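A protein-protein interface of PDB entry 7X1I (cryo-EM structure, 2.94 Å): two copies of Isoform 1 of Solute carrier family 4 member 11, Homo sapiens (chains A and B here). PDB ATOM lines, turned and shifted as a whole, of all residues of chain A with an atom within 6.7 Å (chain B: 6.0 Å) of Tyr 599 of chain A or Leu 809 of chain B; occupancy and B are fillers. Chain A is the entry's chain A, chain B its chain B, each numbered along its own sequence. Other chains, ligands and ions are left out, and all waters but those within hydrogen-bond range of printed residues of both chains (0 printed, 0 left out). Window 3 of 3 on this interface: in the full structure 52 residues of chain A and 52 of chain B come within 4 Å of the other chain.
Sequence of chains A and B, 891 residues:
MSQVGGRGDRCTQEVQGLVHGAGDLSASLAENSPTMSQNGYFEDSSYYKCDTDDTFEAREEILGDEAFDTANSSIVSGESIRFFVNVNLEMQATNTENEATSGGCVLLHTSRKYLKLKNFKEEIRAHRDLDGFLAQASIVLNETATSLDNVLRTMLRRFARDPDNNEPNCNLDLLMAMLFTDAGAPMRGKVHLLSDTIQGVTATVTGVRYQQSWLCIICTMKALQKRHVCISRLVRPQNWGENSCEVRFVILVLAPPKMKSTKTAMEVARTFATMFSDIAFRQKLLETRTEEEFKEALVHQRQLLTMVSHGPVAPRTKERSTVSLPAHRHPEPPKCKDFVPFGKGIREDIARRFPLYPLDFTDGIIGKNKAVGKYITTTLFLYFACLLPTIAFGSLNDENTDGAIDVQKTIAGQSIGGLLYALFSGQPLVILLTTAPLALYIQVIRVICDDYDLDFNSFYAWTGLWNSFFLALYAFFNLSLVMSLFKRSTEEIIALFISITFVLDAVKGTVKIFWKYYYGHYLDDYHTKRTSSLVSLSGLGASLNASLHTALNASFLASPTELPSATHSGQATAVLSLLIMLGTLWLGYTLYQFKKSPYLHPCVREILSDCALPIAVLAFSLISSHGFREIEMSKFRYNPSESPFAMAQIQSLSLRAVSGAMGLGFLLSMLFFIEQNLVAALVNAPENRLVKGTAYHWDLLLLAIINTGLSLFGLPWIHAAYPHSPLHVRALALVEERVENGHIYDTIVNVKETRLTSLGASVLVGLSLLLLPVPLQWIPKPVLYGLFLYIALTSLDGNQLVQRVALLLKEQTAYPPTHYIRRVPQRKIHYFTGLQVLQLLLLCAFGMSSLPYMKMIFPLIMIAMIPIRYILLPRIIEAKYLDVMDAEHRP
The backbone NH (N) of Glu 811 of chain B lies within hydrogen-bond range of the backbone carbonyl oxygen (O) of Pro 598 of chain A.
The backbone carbonyl oxygen (O) of Tyr 599 of chain A sits close to the backbone carbonyl oxygen (O) of Leu 809 of chain B (2.6 Å).
The side-chain carboxylate (OE1) of Glu 811 of chain B lies within salt-bridge range of the guanidinium group (NH2) of Arg 605 of chain A.
No position is printed for both chains.
Tyr 599 of chain A touches just these residues of chain B: Ala 806, Leu 809 and Lys 810.
Leu 809 of chain B touches one residue of chain A.
Of the printed residues of chain B, Arg 605 of chain A touches Glu 811.
Printed residues of chain B within 4 Å of Pro 598 of chain A: Lys 810 (3.0 Å) and Glu 811 (2.6 Å).
Printed residues of chain A within 4 Å of Glu 811 of chain B: Pro 598, Leu 600 and Arg 605.
Val 805 of chain B touches none of the printed residues of chain A.
The nearest residue of chain B that does not touch Tyr 599 of chain A is Glu 811 of chain B (4.7 Å).
Of the 8 printed residues of chain B, 4 touch a printed residue of chain A.
Of the 7 printed residues of chain A, 4 touch a printed residue of chain B.
Hydrophobic or aromatic side chains of chain A that line the printed part of chain B: Pro 598 and Tyr 599.
Among the printed residues, 7 pairs touch across the chains.
The guanidinium group (NE) of Arg 605 of chain A is in hydrogen-bond range of the backbone carbonyl oxygen (O) of Ser 597 of chain A (2.8 Å).
Among the printed residues, pairs that only touch across the chains: Pro 598 of chain A with Lys 810 of chain B (3.0 Å), Tyr 599 of chain A with Lys 810 of chain B (3.6 Å), Tyr 599 of chain A with Ala 806 of chain B (3.8 Å) and Leu 600 of chain A with Glu 811 of chain B (3.9 Å).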
ATOM      1  N   PHE A 594      -1.557 -27.342  -4.961  1.00  0.00           N
ATOM      2  CA  PHE A 594      -0.978 -27.633  -3.655  1.00  0.00           C
ATOM      3  C   PHE A 594      -0.287 -28.990  -3.615  1.00  0.00           C
ATOM      4  O   PHE A 594       0.587 -29.201  -2.768  1.00  0.00           O
ATOM      5  CB  PHE A 594      -2.063 -27.563  -2.579  1.00  0.00           C
ATOM      6  CG  PHE A 594      -1.536 -27.664  -1.178  1.00  0.00           C
ATOM      7  CD1 PHE A 594      -0.814 -26.623  -0.617  1.00  0.00           C
ATOM      8  CD2 PHE A 594      -1.772 -28.795  -0.413  1.00  0.00           C
ATOM      9  CE1 PHE A 594      -0.330 -26.710   0.674  1.00  0.00           C
ATOM     10  CE2 PHE A 594      -1.292 -28.889   0.880  1.00  0.00           C
ATOM     11  CZ  PHE A 594      -0.569 -27.844   1.424  1.00  0.00           C
ATOM     12  N   SER A 597       3.733 -29.064  -3.644  1.00  0.00           N
ATOM     13  CA  SER A 597       4.334 -28.262  -2.593  1.00  0.00           C
ATOM     14  C   SER A 597       4.910 -29.170  -1.518  1.00  0.00           C
ATOM     15  O   SER A 597       4.496 -30.326  -1.381  1.00  0.00           O
ATOM     16  CB  SER A 597       3.303 -27.305  -1.973  1.00  0.00           C
ATOM     17  OG  SER A 597       2.180 -28.015  -1.480  1.00  0.00           O
ATOM     18  N   PRO A 598       5.896 -28.689  -0.763  1.00  0.00           N
ATOM     19  CA  PRO A 598       6.437 -29.460   0.367  1.00  0.00           C
ATOM     20  C   PRO A 598       5.852 -29.113   1.730  1.00  0.00           C
ATOM     21  O   PRO A 598       6.437 -29.511   2.742  1.00  0.00           O
ATOM     22  CB  PRO A 598       7.923 -29.085   0.321  1.00  0.00           C
ATOM     23  CG  PRO A 598       7.906 -27.661  -0.124  1.00  0.00           C
ATOM     24  CD  PRO A 598       6.737 -27.519  -1.076  1.00  0.00           C
ATOM     25  N   TYR A 599       4.732 -28.394   1.796  1.00  0.00           N
ATOM     26  CA  TYR A 599       4.282 -27.764   3.031  1.00  0.00           C
ATOM     27  C   TYR A 599       3.481 -28.688   3.943  1.00  0.00           C
ATOM     28  O   TYR A 599       3.065 -28.249   5.019  1.00  0.00           O
ATOM     29  CB  TYR A 599       3.447 -26.519   2.715  1.00  0.00           C
ATOM     30  CG  TYR A 599       4.256 -25.353   2.198  1.00  0.00           C
ATOM     31  CD1 TYR A 599       5.031 -24.586   3.059  1.00  0.00           C
ATOM     32  CD2 TYR A 599       4.243 -25.015   0.851  1.00  0.00           C
ATOM     33  CE1 TYR A 599       5.774 -23.519   2.593  1.00  0.00           C
ATOM     34  CE2 TYR A 599       4.983 -23.947   0.376  1.00  0.00           C
ATOM     35  CZ  TYR A 599       5.746 -23.204   1.252  1.00  0.00           C
ATOM     36  OH  TYR A 599       6.485 -22.139   0.789  1.00  0.00           O
ATOM     37  N   LEU A 600       3.265 -29.945   3.564  1.00  0.00           N
ATOM     38  CA  LEU A 600       2.480 -30.848   4.397  1.00  0.00           C
ATOM     39  C   LEU A 600       2.969 -32.277   4.193  1.00  0.00           C
ATOM     40  O   LEU A 600       3.834 -32.549   3.354  1.00  0.00           O
ATOM     41  CB  LEU A 600       0.983 -30.739   4.089  1.00  0.00           C
ATOM     42  CG  LEU A 600       0.171 -29.657   4.807  1.00  0.00           C
ATOM     43  CD1 LEU A 600      -1.289 -29.741   4.399  1.00  0.00           C
ATOM     44  CD2 LEU A 600       0.310 -29.782   6.320  1.00  0.00           C
ATOM     45  N   HIS A 601       2.413 -33.186   4.989  1.00  0.00           N
ATOM     46  CA  HIS A 601       2.672 -34.605   4.809  1.00  0.00           C
ATOM     47  C   HIS A 601       2.099 -35.062   3.469  1.00  0.00           C
ATOM     48  O   HIS A 601       1.013 -34.616   3.077  1.00  0.00           O
ATOM     49  CB  HIS A 601       2.054 -35.405   5.958  1.00  0.00           C
ATOM     50  CG  HIS A 601       2.349 -36.872   5.909  1.00  0.00           C
ATOM     51  ND1 HIS A 601       3.605 -37.387   6.144  1.00  0.00           N
ATOM     52  CD2 HIS A 601       1.548 -37.933   5.658  1.00  0.00           C
ATOM     53  CE1 HIS A 601       3.565 -38.703   6.033  1.00  0.00           C
ATOM     54  NE2 HIS A 601       2.329 -39.060   5.738  1.00  0.00           N
ATOM     55  N   ARG A 605      -1.400 -33.954   2.157  1.00  0.00           N
ATOM     56  CA  ARG A 605      -1.364 -33.033   1.027  1.00  0.00           C
ATOM     57  C   ARG A 605      -2.089 -33.608  -0.183  1.00  0.00           C
ATOM     58  O   ARG A 605      -2.794 -32.884  -0.895  1.00  0.00           O
ATOM     59  CB  ARG A 605       0.084 -32.694   0.678  1.00  0.00           C
ATOM     60  CG  ARG A 605       0.234 -31.744  -0.491  1.00  0.00           C
ATOM     61  CD  ARG A 605       1.661 -31.249  -0.616  1.00  0.00           C
ATOM     62  NE  ARG A 605       2.589 -32.300  -1.020  1.00  0.00           N
ATOM     63  CZ  ARG A 605       3.403 -32.939  -0.193  1.00  0.00           C
ATOM     64  NH1 ARG A 605       3.438 -32.661   1.098  1.00  0.00           N
ATOM     65  NH2 ARG A 605       4.210 -33.879  -0.677  1.00  0.00           N
ATOM     66  N   ARG B 804      11.474 -19.708   8.328  1.00  0.00           N
ATOM     67  CA  ARG B 804      11.486 -20.733   9.366  1.00  0.00           C
ATOM     68  C   ARG B 804      10.086 -21.057   9.875  1.00  0.00           C
ATOM     69  O   ARG B 804       9.846 -22.180  10.331  1.00  0.00           O
ATOM     70  CB  ARG B 804      12.387 -20.299  10.524  1.00  0.00           C
ATOM     71  CG  ARG B 804      13.868 -20.489  10.239  1.00  0.00           C
ATOM     72  CD  ARG B 804      14.735 -20.158  11.444  1.00  0.00           C
ATOM     73  NE  ARG B 804      14.868 -18.721  11.651  1.00  0.00           N
ATOM     74  CZ  ARG B 804      14.153 -18.018  12.519  1.00  0.00           C
ATOM     75  NH1 ARG B 804      13.240 -18.588  13.287  1.00  0.00           N
ATOM     76  NH2 ARG B 804      14.365 -16.709  12.623  1.00  0.00           N
ATOM     77  N   VAL B 805       9.158 -20.099   9.819  1.00  0.00           N
ATOM     78  CA  VAL B 805       7.766 -20.403  10.149  1.00  0.00           C
ATOM     79  C   VAL B 805       7.193 -21.398   9.147  1.00  0.00           C
ATOM     80  O   VAL B 805       6.529 -22.372   9.525  1.00  0.00           O
ATOM     81  CB  VAL B 805       6.933 -19.109  10.211  1.00  0.00           C
ATOM     82  CG1 VAL B 805       5.446 -19.426  10.153  1.00  0.00           C
ATOM     83  CG2 VAL B 805       7.259 -18.336  11.479  1.00  0.00           C
ATOM     84  N   ALA B 806       7.451 -21.176   7.856  1.00  0.00           N
ATOM     85  CA  ALA B 806       7.028 -22.131   6.838  1.00  0.00           C
ATOM     86  C   ALA B 806       7.774 -23.452   6.963  1.00  0.00           C
ATOM     87  O   ALA B 806       7.257 -24.495   6.549  1.00  0.00           O
ATOM     88  CB  ALA B 806       7.229 -21.537   5.444  1.00  0.00           C
ATOM     89  N   LEU B 807       8.988 -23.424   7.522  1.00  0.00           N
ATOM     90  CA  LEU B 807       9.756 -24.650   7.711  1.00  0.00           C
ATOM     91  C   LEU B 807       9.034 -25.631   8.626  1.00  0.00           C
ATOM     92  O   LEU B 807       9.173 -26.849   8.463  1.00  0.00           O
ATOM     93  CB  LEU B 807      11.139 -24.318   8.274  1.00  0.00           C
ATOM     94  CG  LEU B 807      12.190 -25.426   8.235  1.00  0.00           C
ATOM     95  CD1 LEU B 807      12.569 -25.731   6.797  1.00  0.00           C
ATOM     96  CD2 LEU B 807      13.417 -25.036   9.043  1.00  0.00           C
ATOM     97  N   LEU B 808       8.275 -25.122   9.601  1.00  0.00           N
ATOM     98  CA  LEU B 808       7.489 -25.996  10.468  1.00  0.00           C
ATOM     99  C   LEU B 808       6.446 -26.770   9.672  1.00  0.00           C
ATOM    100  O   LEU B 808       6.257 -27.973   9.888  1.00  0.00           O
ATOM    101  CB  LEU B 808       6.817 -25.175  11.567  1.00  0.00           C
ATOM    102  CG  LEU B 808       7.725 -24.505  12.599  1.00  0.00           C
ATOM    103  CD1 LEU B 808       6.946 -23.483  13.408  1.00  0.00           C
ATOM    104  CD2 LEU B 808       8.343 -25.547  13.513  1.00  0.00           C
ATOM    105  N   LEU B 809       5.758 -26.099   8.752  1.00  0.00           N
ATOM    106  CA  LEU B 809       4.745 -26.739   7.915  1.00  0.00           C
ATOM    107  C   LEU B 809       5.370 -27.140   6.578  1.00  0.00           C
ATOM    108  O   LEU B 809       5.057 -26.603   5.514  1.00  0.00           O
ATOM    109  CB  LEU B 809       3.551 -25.807   7.726  1.00  0.00           C
ATOM    110  CG  LEU B 809       2.887 -25.298   9.007  1.00  0.00           C
ATOM    111  CD1 LEU B 809       1.772 -24.315   8.683  1.00  0.00           C
ATOM    112  CD2 LEU B 809       2.361 -26.459   9.835  1.00  0.00           C
ATOM    113  N   LYS B 810       6.276 -28.111   6.660  1.00  0.00           N
ATOM    114  CA  LYS B 810       7.012 -28.562   5.489  1.00  0.00           C
ATOM    115  C   LYS B 810       7.590 -29.942   5.769  1.00  0.00           C
ATOM    116  O   LYS B 810       8.065 -30.206   6.877  1.00  0.00           O
ATOM    117  CB  LYS B 810       8.128 -27.577   5.121  1.00  0.00           C
ATOM    118  CG  LYS B 810       8.866 -27.920   3.840  1.00  0.00           C
ATOM    119  CD  LYS B 810       9.878 -26.842   3.485  1.00  0.00           C
ATOM    120  CE  LYS B 810       9.193 -25.508   3.236  1.00  0.00           C
ATOM    121  NZ  LYS B 810      10.167 -24.431   2.915  1.00  0.00           N
ATOM    122  N   GLU B 811       7.536 -30.812   4.764  1.00  0.00           N
ATOM    123  CA  GLU B 811       8.089 -32.152   4.898  1.00  0.00           C
ATOM    124  C   GLU B 811       9.603 -32.092   5.073  1.00  0.00           C
ATOM    125  O   GLU B 811      10.268 -31.155   4.620  1.00  0.00           O
ATOM    126  CB  GLU B 811       7.734 -32.999   3.676  1.00  0.00           C
ATOM    127  CG  GLU B 811       8.233 -32.432   2.359  1.00  0.00           C
ATOM    128  CD  GLU B 811       7.845 -33.291   1.171  1.00  0.00           C
ATOM    129  OE1 GLU B 811       7.154 -34.311   1.375  1.00  0.00           O
ATOM    130  OE2 GLU B 811       8.232 -32.945   0.035  1.00  0.00           O
